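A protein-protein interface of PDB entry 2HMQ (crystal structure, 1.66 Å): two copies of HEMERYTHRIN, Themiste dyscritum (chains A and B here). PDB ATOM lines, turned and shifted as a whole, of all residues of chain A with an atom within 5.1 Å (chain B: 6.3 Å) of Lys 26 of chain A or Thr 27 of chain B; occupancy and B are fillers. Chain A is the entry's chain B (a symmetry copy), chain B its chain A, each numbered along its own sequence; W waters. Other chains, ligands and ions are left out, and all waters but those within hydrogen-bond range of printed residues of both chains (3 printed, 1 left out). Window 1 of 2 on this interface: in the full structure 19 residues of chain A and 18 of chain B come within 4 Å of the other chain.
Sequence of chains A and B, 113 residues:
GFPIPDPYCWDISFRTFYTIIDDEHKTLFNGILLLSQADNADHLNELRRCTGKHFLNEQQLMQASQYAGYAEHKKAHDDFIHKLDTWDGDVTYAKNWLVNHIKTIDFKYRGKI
The side-chain amide oxygen (OD1) of Asn 30 of chain B sits close to the backbone carbonyl oxygen (O) of Trp 10 of chain A, 3.1 Å away. The side-chain amino group (NZ) of Lys 26 of chain A is in salt-bridge range of the side-chain carboxylate (OE1) of Glu 46 of chain B (2.7 Å). The side-chain carboxylate of Asp 23 of chain A is in salt-bridge range of the guanidinium group of Arg 49 of chain B (2.8 Å). The side-chain carboxylate of Asp 23 of chain A lies within hydrogen-bond range of the side-chain sulfur of Cys 50 of chain B, at 3.5 Å. The side-chain sulfur of Cys 50 of chain B is in hydrogen-bond range of the side-chain amino group of Lys 26 of chain A (3.4 Å). NZ of Lys 53 of chain B lies within salt-bridge range of OD1 of Asp 23 of chain A.
OD2 of Asp 23 of chain B is in salt-bridge range of NZ of Lys 26 of chain B (2.9 Å). SG of Cys 50 of chain B sits close to OG1 of Thr 27 of chain B, at 3.8 Å. The backbone carbonyl oxygen (O) of Glu 46 of chain B is in hydrogen-bond range of the side-chain sulfur (SG) of Cys 50 of chain B (3.4 Å). The guanidinium group of Arg 49 of chain B lies within hydrogen-bond range of the side-chain sulfur of Cys 50 of chain B (3.6 Å). NZ of Lys 26 of chain A is in salt-bridge range of OD2 of Asp 23 of chain A (3.0 Å). The backbone carbonyl oxygen (O) of Glu 24 of chain A is in hydrogen-bond range of the side-chain hydroxyl (OG1) of Thr 27 of chain A (2.7 Å).
Among the printed residues, pairs that only touch across the chains: Trp 10 of chain A with Leu 34 of chain B, Lys 26 of chain A with Arg 49 of chain B, Lys 26 of chain A with Asn 30 of chain B, Trp 10 of chain A with Glu 46 of chain B, Asn 30 of chain A with Lys 26 of chain B, Asp 23 of chain A with Thr 27 of chain B, Lys 26 of chain A with Thr 27 of chain B and Thr 27 of chain A with Asp 23 of chain B.
Printed residues of chain B within 4 Å of Trp 10 of chain A: Asn 30, Leu 34 and Glu 46. Of the printed residues of chain B, Asn 30 of chain A touches Lys 26 (3.8 Å). Of the printed residues of chain A, Lys 26 of chain B touches Asn 30 (3.8 Å). Of the printed residues of chain A, Cys 50 of chain B touches Asp 23 and Lys 26. The nearest printed residue of chain A that does not touch Thr 27 of chain B is Thr 27 of chain A (5.1 Å).
Of the 19 printed residues of chain B, 9 touch a printed residue of chain A. Of the 10 printed residues of chain A, 5 touch a printed residue of chain B. Hydrophobic or aromatic side chains of chain A within 4 Å of the printed part of chain B: Trp 10.
Asp 23 of chain A touches Thr 27 of chain B, and with the chains exchanged Thr 27 of chain A touches Asp 23 of chain B. Lys 26 of chain A touches Thr 27 of chain B, but with the chains exchanged Thr 27 of chain A does not touch Lys 26 of chain B (4.03 Å). Lys 26 of chain A touches Asn 30 of chain B, and with the chains exchanged Asn 30 of chain A touches Lys 26 of chain B. 9 positions are printed for both chains. Of the 14 pairs that touch across the chains among the printed residues, 4 have their exchanged pair printed and touching as well.
Water W2 lies within hydrogen-bond range of ND2 of Asn 30 of chain A (2.8 Å), NZ of Lys 26 of chain B (2.8 Å) and O of Thr 27 of chain A (2.9 Å). Water W3 lies within hydrogen-bond range of OD2 of Asp 22 of chain A (2.8 Å) and OE1 of Glu 46 of chain B (2.9 Å). Water W1 bridges the side-chain carboxylate (OD1) of Asp 23 of chain A (2.9 Å) and the side-chain amino group (NZ) of Lys 53 of chain B (3.0 Å).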
ATOM      1  N   TRP A  10       0.696  -1.373  14.586  1.00  0.00           N
ATOM      2  CA  TRP A  10       1.457  -2.047  13.542  1.00  0.00           C
ATOM      3  C   TRP A  10       1.082  -1.526  12.187  1.00  0.00           C
ATOM      4  O   TRP A  10      -0.143  -1.271  11.886  1.00  0.00           O
ATOM      5  CB  TRP A  10       1.129  -3.590  13.740  1.00  0.00           C
ATOM      6  CG  TRP A  10       1.898  -4.492  12.783  1.00  0.00           C
ATOM      7  CD1 TRP A  10       3.095  -5.104  13.080  1.00  0.00           C
ATOM      8  CD2 TRP A  10       1.556  -4.883  11.486  1.00  0.00           C
ATOM      9  NE1 TRP A  10       3.488  -5.887  12.033  1.00  0.00           N
ATOM     10  CE2 TRP A  10       2.530  -5.809  11.033  1.00  0.00           C
ATOM     11  CE3 TRP A  10       0.470  -4.656  10.630  1.00  0.00           C
ATOM     12  CZ2 TRP A  10       2.543  -6.366   9.756  1.00  0.00           C
ATOM     13  CZ3 TRP A  10       0.460  -5.210   9.400  1.00  0.00           C
ATOM     14  CH2 TRP A  10       1.465  -6.066   8.944  1.00  0.00           C
ATOM     15  N   ASP A  22       4.385 -11.697  12.252  1.00  0.00           N
ATOM     16  CA  ASP A  22       3.709 -10.421  12.085  1.00  0.00           C
ATOM     17  C   ASP A  22       2.539 -10.357  13.049  1.00  0.00           C
ATOM     18  O   ASP A  22       2.233  -9.291  13.569  1.00  0.00           O
ATOM     19  CB  ASP A  22       3.272 -10.231  10.638  1.00  0.00           C
ATOM     20  CG  ASP A  22       4.508 -10.025   9.710  1.00  0.00           C
ATOM     21  OD1 ASP A  22       5.570  -9.734  10.181  1.00  0.00           O
ATOM     22  OD2 ASP A  22       4.261 -10.126   8.539  1.00  0.00           O
ATOM     23  N   ASP A  23       1.706 -11.395  13.080  1.00  0.00           N
ATOM     24  CA  ASP A  23       0.512 -11.393  13.970  1.00  0.00           C
ATOM     25  C   ASP A  23       0.979 -11.265  15.397  1.00  0.00           C
ATOM     26  O   ASP A  23       0.296 -10.515  16.135  1.00  0.00           O
ATOM     27  CB  ASP A  23      -0.345 -12.582  13.719  1.00  0.00           C
ATOM     28  CG  ASP A  23      -1.110 -12.539  12.451  1.00  0.00           C
ATOM     29  OD1 ASP A  23      -1.666 -13.585  12.044  1.00  0.00           O
ATOM     30  OD2 ASP A  23      -1.117 -11.522  11.745  1.00  0.00           O
ATOM     31  N   GLU A  24       1.987 -11.937  15.875  1.00  0.00           N
ATOM     32  CA  GLU A  24       2.469 -11.695  17.225  1.00  0.00           C
ATOM     33  C   GLU A  24       2.924 -10.246  17.451  1.00  0.00           C
ATOM     34  O   GLU A  24       2.694  -9.660  18.527  1.00  0.00           O
ATOM     35  CB  GLU A  24       3.582 -12.650  17.581  1.00  0.00           C
ATOM     36  CG  GLU A  24       3.015 -14.059  17.769  1.00  0.00           C
ATOM     37  CD  GLU A  24       4.025 -15.127  17.984  1.00  0.00           C
ATOM     38  OE1 GLU A  24       3.645 -16.279  18.251  1.00  0.00           O
ATOM     39  OE2 GLU A  24       5.238 -14.798  17.977  1.00  0.00           O
ATOM     40  N   HIS A  25       3.649  -9.708  16.478  1.00  0.00           N
ATOM     41  CA  HIS A  25       4.098  -8.275  16.606  1.00  0.00           C
ATOM     42  C   HIS A  25       2.955  -7.335  16.777  1.00  0.00           C
ATOM     43  O   HIS A  25       3.096  -6.311  17.519  1.00  0.00           O
ATOM     44  CB  HIS A  25       4.969  -7.872  15.361  1.00  0.00           C
ATOM     45  CG  HIS A  25       6.363  -8.420  15.456  1.00  0.00           C
ATOM     46  ND1 HIS A  25       7.119  -8.434  14.294  1.00  0.00           N
ATOM     47  CD2 HIS A  25       7.096  -8.979  16.398  1.00  0.00           C
ATOM     48  CE1 HIS A  25       8.263  -8.983  14.593  1.00  0.00           C
ATOM     49  NE2 HIS A  25       8.358  -9.292  15.862  1.00  0.00           N
ATOM     50  N   LYS A  26       1.824  -7.507  16.118  1.00  0.00           N
ATOM     51  CA  LYS A  26       0.636  -6.658  16.229  1.00  0.00           C
ATOM     52  C   LYS A  26       0.204  -6.598  17.699  1.00  0.00           C
ATOM     53  O   LYS A  26      -0.224  -5.584  18.185  1.00  0.00           O
ATOM     54  CB  LYS A  26      -0.513  -7.125  15.339  1.00  0.00           C
ATOM     55  CG  LYS A  26      -0.186  -7.203  13.852  1.00  0.00           C
ATOM     56  CD  LYS A  26      -1.282  -7.847  13.000  1.00  0.00           C
ATOM     57  CE  LYS A  26      -0.833  -8.005  11.580  1.00  0.00           C
ATOM     58  NZ  LYS A  26      -1.798  -8.820  10.750  1.00  0.00           N
ATOM     59  N   THR A  27       0.373  -7.724  18.436  1.00  0.00           N
ATOM     60  CA  THR A  27      -0.007  -7.713  19.840  1.00  0.00           C
ATOM     61  C   THR A  27       0.953  -6.896  20.686  1.00  0.00           C
ATOM     62  O   THR A  27       0.456  -6.350  21.726  1.00  0.00           O
ATOM     63  CB  THR A  27      -0.187  -9.175  20.418  1.00  0.00           C
ATOM     64  OG1 THR A  27       1.117  -9.716  20.672  1.00  0.00           O
ATOM     65  CG2 THR A  27      -1.061 -10.030  19.487  1.00  0.00           C
ATOM     66  N   LEU A  28       2.203  -6.786  20.335  1.00  0.00           N
ATOM     67  CA  LEU A  28       3.191  -5.987  21.123  1.00  0.00           C
ATOM     68  C   LEU A  28       2.867  -4.493  20.853  1.00  0.00           C
ATOM     69  O   LEU A  28       2.951  -3.718  21.801  1.00  0.00           O
ATOM     70  CB  LEU A  28       4.581  -6.415  20.836  1.00  0.00           C
ATOM     71  CG  LEU A  28       5.136  -7.782  20.882  1.00  0.00           C
ATOM     72  CD1 LEU A  28       6.650  -7.732  21.228  1.00  0.00           C
ATOM     73  CD2 LEU A  28       4.550  -8.651  21.922  1.00  0.00           C
ATOM     74  N   PHE A  29       2.599  -4.115  19.627  1.00  0.00           N
ATOM     75  CA  PHE A  29       2.177  -2.762  19.318  1.00  0.00           C
ATOM     76  C   PHE A  29       0.974  -2.400  20.225  1.00  0.00           C
ATOM     77  O   PHE A  29       0.927  -1.327  20.838  1.00  0.00           O
ATOM     78  CB  PHE A  29       1.810  -2.448  17.865  1.00  0.00           C
ATOM     79  CG  PHE A  29       3.015  -2.176  17.012  1.00  0.00           C
ATOM     80  CD1 PHE A  29       3.729  -3.203  16.448  1.00  0.00           C
ATOM     81  CD2 PHE A  29       3.436  -0.830  16.785  1.00  0.00           C
ATOM     82  CE1 PHE A  29       4.847  -2.983  15.653  1.00  0.00           C
ATOM     83  CE2 PHE A  29       4.573  -0.564  16.008  1.00  0.00           C
ATOM     84  CZ  PHE A  29       5.278  -1.649  15.461  1.00  0.00           C
ATOM     85  N   ASN A  30      -0.045  -3.179  20.230  1.00  0.00           N
ATOM     86  CA  ASN A  30      -1.268  -2.920  21.042  1.00  0.00           C
ATOM     87  C   ASN A  30      -0.912  -2.839  22.501  1.00  0.00           C
ATOM     88  O   ASN A  30      -1.455  -1.954  23.157  1.00  0.00           O
ATOM     89  CB  ASN A  30      -2.323  -3.975  20.717  1.00  0.00           C
ATOM     90  CG  ASN A  30      -3.511  -3.901  21.645  1.00  0.00           C
ATOM     91  OD1 ASN A  30      -4.344  -3.056  21.290  1.00  0.00           O
ATOM     92  ND2 ASN A  30      -3.497  -4.646  22.704  1.00  0.00           N
ATOM     93  N   ASP B  22      -8.174 -13.619  22.307  1.00  0.00           N
ATOM     94  CA  ASP B  22      -7.923 -12.168  22.467  1.00  0.00           C
ATOM     95  C   ASP B  22      -6.780 -11.745  21.522  1.00  0.00           C
ATOM     96  O   ASP B  22      -6.916 -10.680  20.924  1.00  0.00           O
ATOM     97  CB  ASP B  22      -7.590 -11.769  23.930  1.00  0.00           C
ATOM     98  CG  ASP B  22      -8.830 -11.962  24.837  1.00  0.00           C
ATOM     99  OD1 ASP B  22      -9.965 -12.021  24.396  1.00  0.00           O
ATOM    100  OD2 ASP B  22      -8.491 -11.993  26.027  1.00  0.00           O
ATOM    101  N   ASP B  23      -5.683 -12.445  21.488  1.00  0.00           N
ATOM    102  CA  ASP B  23      -4.520 -12.135  20.585  1.00  0.00           C
ATOM    103  C   ASP B  23      -5.005 -12.166  19.171  1.00  0.00           C
ATOM    104  O   ASP B  23      -4.656 -11.209  18.435  1.00  0.00           O
ATOM    105  CB  ASP B  23      -3.366 -13.022  20.906  1.00  0.00           C
ATOM    106  CG  ASP B  23      -2.678 -12.744  22.193  1.00  0.00           C
ATOM    107  OD1 ASP B  23      -1.845 -13.543  22.613  1.00  0.00           O
ATOM    108  OD2 ASP B  23      -2.963 -11.689  22.836  1.00  0.00           O
ATOM    109  N   GLU B  24      -5.801 -13.079  18.704  1.00  0.00           N
ATOM    110  CA  GLU B  24      -6.314 -12.986  17.341  1.00  0.00           C
ATOM    111  C   GLU B  24      -7.156 -11.779  17.074  1.00  0.00           C
ATOM    112  O   GLU B  24      -7.155 -11.129  16.020  1.00  0.00           O
ATOM    113  CB  GLU B  24      -7.130 -14.270  16.984  1.00  0.00           C
ATOM    114  CG  GLU B  24      -6.232 -15.507  16.937  1.00  0.00           C
ATOM    115  CD  GLU B  24      -6.859 -16.828  16.601  1.00  0.00           C
ATOM    116  OE1 GLU B  24      -6.085 -17.769  16.327  1.00  0.00           O
ATOM    117  OE2 GLU B  24      -8.091 -16.894  16.615  1.00  0.00           O
ATOM    118  N   HIS B  25      -8.042 -11.486  18.053  1.00  0.00           N
ATOM    119  CA  HIS B  25      -8.919 -10.320  17.942  1.00  0.00           C
ATOM    120  C   HIS B  25      -8.118  -9.027  17.730  1.00  0.00           C
ATOM    121  O   HIS B  25      -8.546  -8.212  16.902  1.00  0.00           O
ATOM    122  CB  HIS B  25      -9.839 -10.162  19.169  1.00  0.00           C
ATOM    123  CG  HIS B  25     -10.980 -11.142  19.149  1.00  0.00           C
ATOM    124  ND1 HIS B  25     -11.721 -11.365  20.307  1.00  0.00           N
ATOM    125  CD2 HIS B  25     -11.549 -11.881  18.184  1.00  0.00           C
ATOM    126  CE1 HIS B  25     -12.694 -12.158  20.020  1.00  0.00           C
ATOM    127  NE2 HIS B  25     -12.639 -12.566  18.778  1.00  0.00           N
ATOM    128  N   LYS B  26      -7.016  -8.879  18.386  1.00  0.00           N
ATOM    129  CA  LYS B  26      -6.154  -7.696  18.224  1.00  0.00           C
ATOM    130  C   LYS B  26      -5.784  -7.535  16.777  1.00  0.00           C
ATOM    131  O   LYS B  26      -5.674  -6.415  16.273  1.00  0.00           O
ATOM    132  CB  LYS B  26      -4.944  -7.822  19.131  1.00  0.00           C
ATOM    133  CG  LYS B  26      -5.190  -7.786  20.632  1.00  0.00           C
ATOM    134  CD  LYS B  26      -4.021  -8.166  21.489  1.00  0.00           C
ATOM    135  CE  LYS B  26      -4.400  -8.455  22.913  1.00  0.00           C
ATOM    136  NZ  LYS B  26      -3.300  -8.936  23.723  1.00  0.00           N
ATOM    137  N   THR B  27      -5.572  -8.640  16.047  1.00  0.00           N
ATOM    138  CA  THR B  27      -5.164  -8.571  14.631  1.00  0.00           C
ATOM    139  C   THR B  27      -6.338  -8.166  13.837  1.00  0.00           C
ATOM    140  O   THR B  27      -6.111  -7.487  12.818  1.00  0.00           O
ATOM    141  CB  THR B  27      -4.479  -9.904  14.115  1.00  0.00           C
ATOM    142  OG1 THR B  27      -5.597 -10.864  13.919  1.00  0.00           O
ATOM    143  CG2 THR B  27      -3.418 -10.510  14.938  1.00  0.00           C
ATOM    144  N   LEU B  28      -7.573  -8.356  14.189  1.00  0.00           N
ATOM    145  CA  LEU B  28      -8.739  -7.956  13.430  1.00  0.00           C
ATOM    146  C   LEU B  28      -8.930  -6.396  13.650  1.00  0.00           C
ATOM    147  O   LEU B  28      -9.267  -5.787  12.651  1.00  0.00           O
ATOM    148  CB  LEU B  28      -9.932  -8.745  13.729  1.00  0.00           C
ATOM    149  CG  LEU B  28      -9.960 -10.268  13.615  1.00  0.00           C
ATOM    150  CD1 LEU B  28     -11.344 -10.801  13.939  1.00  0.00           C
ATOM    151  CD2 LEU B  28      -9.549 -10.599  12.208  1.00  0.00           C
ATOM    152  N   PHE B  29      -8.780  -5.926  14.838  1.00  0.00           N
ATOM    153  CA  PHE B  29      -8.819  -4.457  15.102  1.00  0.00           C
ATOM    154  C   PHE B  29      -7.783  -3.796  14.148  1.00  0.00           C
ATOM    155  O   PHE B  29      -8.064  -2.852  13.428  1.00  0.00           O
ATOM    156  CB  PHE B  29      -8.540  -4.149  16.547  1.00  0.00           C
ATOM    157  CG  PHE B  29      -9.796  -4.243  17.413  1.00  0.00           C
ATOM    158  CD1 PHE B  29     -10.193  -5.452  17.955  1.00  0.00           C
ATOM    159  CD2 PHE B  29     -10.610  -3.096  17.561  1.00  0.00           C
ATOM    160  CE1 PHE B  29     -11.344  -5.563  18.727  1.00  0.00           C
ATOM    161  CE2 PHE B  29     -11.786  -3.176  18.291  1.00  0.00           C
ATOM    162  CZ  PHE B  29     -12.115  -4.394  18.906  1.00  0.00           C
ATOM    163  N   ASN B  30      -6.567  -4.313  14.224  1.00  0.00           N
ATOM    164  CA  ASN B  30      -5.463  -3.762  13.390  1.00  0.00           C
ATOM    165  C   ASN B  30      -5.858  -3.815  11.961  1.00  0.00           C
ATOM    166  O   ASN B  30      -5.636  -2.741  11.317  1.00  0.00           O
ATOM    167  CB  ASN B  30      -4.143  -4.454  13.679  1.00  0.00           C
ATOM    168  CG  ASN B  30      -2.990  -3.936  12.817  1.00  0.00           C
ATOM    169  OD1 ASN B  30      -2.466  -2.851  13.165  1.00  0.00           O
ATOM    170  ND2 ASN B  30      -2.672  -4.634  11.787  1.00  0.00           N
ATOM    171  N   GLY B  31      -6.361  -4.843  11.349  1.00  0.00           N
ATOM    172  CA  GLY B  31      -6.724  -4.933   9.952  1.00  0.00           C
ATOM    173  C   GLY B  31      -7.727  -3.819   9.580  1.00  0.00           C
ATOM    174  O   GLY B  31      -7.569  -3.262   8.517  1.00  0.00           O
ATOM    175  N   ILE B  32      -8.723  -3.578  10.439  1.00  0.00           N
ATOM    176  CA  ILE B  32      -9.719  -2.556  10.159  1.00  0.00           C
ATOM    177  C   ILE B  32      -9.072  -1.200  10.347  1.00  0.00           C
ATOM    178  O   ILE B  32      -9.400  -0.326   9.531  1.00  0.00           O
ATOM    179  CB  ILE B  32     -11.029  -2.760  10.974  1.00  0.00           C
ATOM    180  CG1 ILE B  32     -11.692  -4.089  10.576  1.00  0.00           C
ATOM    181  CG2 ILE B  32     -12.031  -1.609  10.735  1.00  0.00           C
ATOM    182  CD1 ILE B  32     -12.799  -4.530  11.606  1.00  0.00           C
ATOM    183  N   LEU B  34      -5.941  -0.304   9.598  1.00  0.00           N
ATOM    184  CA  LEU B  34      -5.174  -0.090   8.353  1.00  0.00           C
ATOM    185  C   LEU B  34      -6.118   0.271   7.233  1.00  0.00           C
ATOM    186  O   LEU B  34      -5.746   1.155   6.459  1.00  0.00           O
ATOM    187  CB  LEU B  34      -4.338  -1.313   8.048  1.00  0.00           C
ATOM    188  CG  LEU B  34      -3.256  -1.707   9.005  1.00  0.00           C
ATOM    189  CD1 LEU B  34      -2.700  -3.072   8.480  1.00  0.00           C
ATOM    190  CD2 LEU B  34      -2.226  -0.702   9.153  1.00  0.00           C
ATOM    191  N   GLU B  46      -4.419  -8.367   4.433  1.00  0.00           N
ATOM    192  CA  GLU B  46      -4.041  -8.557   5.804  1.00  0.00           C
ATOM    193  C   GLU B  46      -5.265  -8.854   6.713  1.00  0.00           C
ATOM    194  O   GLU B  46      -5.352  -9.805   7.482  1.00  0.00           O
ATOM    195  CB  GLU B  46      -3.352  -7.323   6.387  1.00  0.00           C
ATOM    196  CG  GLU B  46      -2.432  -7.571   7.529  1.00  0.00           C
ATOM    197  CD  GLU B  46      -1.264  -8.466   7.451  1.00  0.00           C
ATOM    198  OE1 GLU B  46      -0.693  -9.074   8.300  1.00  0.00           O
ATOM    199  OE2 GLU B  46      -0.785  -8.499   6.262  1.00  0.00           O
ATOM    200  N   LEU B  47      -6.277  -8.011   6.628  1.00  0.00           N
ATOM    201  CA  LEU B  47      -7.501  -8.199   7.350  1.00  0.00           C
ATOM    202  C   LEU B  47      -8.137  -9.523   6.935  1.00  0.00           C
ATOM    203  O   LEU B  47      -8.636 -10.252   7.827  1.00  0.00           O
ATOM    204  CB  LEU B  47      -8.510  -7.023   7.128  1.00  0.00           C
ATOM    205  CG  LEU B  47      -9.902  -7.213   7.810  1.00  0.00           C
ATOM    206  CD1 LEU B  47      -9.689  -7.379   9.301  1.00  0.00           C
ATOM    207  CD2 LEU B  47     -10.825  -6.057   7.490  1.00  0.00           C
ATOM    208  N   ARG B  49      -6.935 -12.309   5.609  1.00  0.00           N
ATOM    209  CA  ARG B  49      -6.171 -13.456   6.097  1.00  0.00           C
ATOM    210  C   ARG B  49      -6.463 -13.614   7.615  1.00  0.00           C
ATOM    211  O   ARG B  49      -6.829 -14.718   8.051  1.00  0.00           O
ATOM    212  CB  ARG B  49      -4.665 -13.279   5.908  1.00  0.00           C
ATOM    213  CG  ARG B  49      -3.864 -14.424   6.436  1.00  0.00           C
ATOM    214  CD  ARG B  49      -2.417 -14.143   6.319  1.00  0.00           C
ATOM    215  NE  ARG B  49      -1.870 -13.041   7.055  1.00  0.00           N
ATOM    216  CZ  ARG B  49      -1.652 -12.976   8.366  1.00  0.00           C
ATOM    217  NH1 ARG B  49      -1.105 -11.928   8.971  1.00  0.00           N
ATOM    218  NH2 ARG B  49      -1.977 -14.046   9.115  1.00  0.00           N
ATOM    219  N   CYS B  50      -6.271 -12.589   8.412  1.00  0.00           N
ATOM    220  CA  CYS B  50      -6.458 -12.646   9.846  1.00  0.00           C
ATOM    221  C   CYS B  50      -7.889 -12.986  10.202  1.00  0.00           C
ATOM    222  O   CYS B  50      -8.053 -13.734  11.161  1.00  0.00           O
ATOM    223  CB  CYS B  50      -5.987 -11.346  10.486  1.00  0.00           C
ATOM    224  SG  CYS B  50      -4.268 -11.076  10.397  1.00  0.00           S
ATOM    225  N   THR B  51      -8.878 -12.570   9.488  1.00  0.00           N
ATOM    226  CA  THR B  51     -10.289 -12.871   9.746  1.00  0.00           C
ATOM    227  C   THR B  51     -10.566 -14.344   9.453  1.00  0.00           C
ATOM    228  O   THR B  51     -11.170 -15.093  10.262  1.00  0.00           O
ATOM    229  CB  THR B  51     -11.257 -11.948   8.953  1.00  0.00           C
ATOM    230  OG1 THR B  51     -10.920 -10.578   9.336  1.00  0.00           O
ATOM    231  CG2 THR B  51     -12.749 -12.239   9.173  1.00  0.00           C
ATOM    232  N   LYS B  53      -8.485 -16.861   9.397  1.00  0.00           N
ATOM    233  CA  LYS B  53      -7.762 -17.659  10.336  1.00  0.00           C
ATOM    234  C   LYS B  53      -8.471 -17.578  11.709  1.00  0.00           C
ATOM    235  O   LYS B  53      -8.704 -18.667  12.330  1.00  0.00           O
ATOM    236  CB  LYS B  53      -6.348 -17.182  10.459  1.00  0.00           C
ATOM    237  CG  LYS B  53      -5.529 -17.917  11.491  1.00  0.00           C
ATOM    238  CD  LYS B  53      -4.152 -17.304  11.672  1.00  0.00           C
ATOM    239  CE  LYS B  53      -4.024 -16.573  12.959  1.00  0.00           C
ATOM    240  NZ  LYS B  53      -3.788 -15.120  12.891  1.00  0.00           N
ATOM    241  N   HIS B  54      -8.835 -16.393  12.185  1.00  0.00           N
ATOM    242  CA  HIS B  54      -9.471 -16.301  13.493  1.00  0.00           C
ATOM    243  C   HIS B  54     -10.810 -17.037  13.477  1.00  0.00           C
ATOM    244  O   HIS B  54     -11.055 -17.770  14.470  1.00  0.00           O
ATOM    245  CB  HIS B  54      -9.689 -14.834  13.897  1.00  0.00           C
ATOM    246  CG  HIS B  54     -10.501 -14.803  15.193  1.00  0.00           C
ATOM    247  ND1 HIS B  54     -10.086 -15.398  16.321  1.00  0.00           N
ATOM    248  CD2 HIS B  54     -11.753 -14.343  15.338  1.00  0.00           C
ATOM    249  CE1 HIS B  54     -11.094 -15.234  17.207  1.00  0.00           C
ATOM    250  NE2 HIS B  54     -12.067 -14.612  16.615  1.00  0.00           N
HETATM  251  O   HOH W   1      -1.048 -16.386  12.569  1.00  0.00           O
HETATM  252  O   HOH W   2      -1.736  -6.591  23.550  1.00  0.00           O
HETATM  253  O   HOH W   3       1.878  -9.632   7.143  1.00  0.00           O
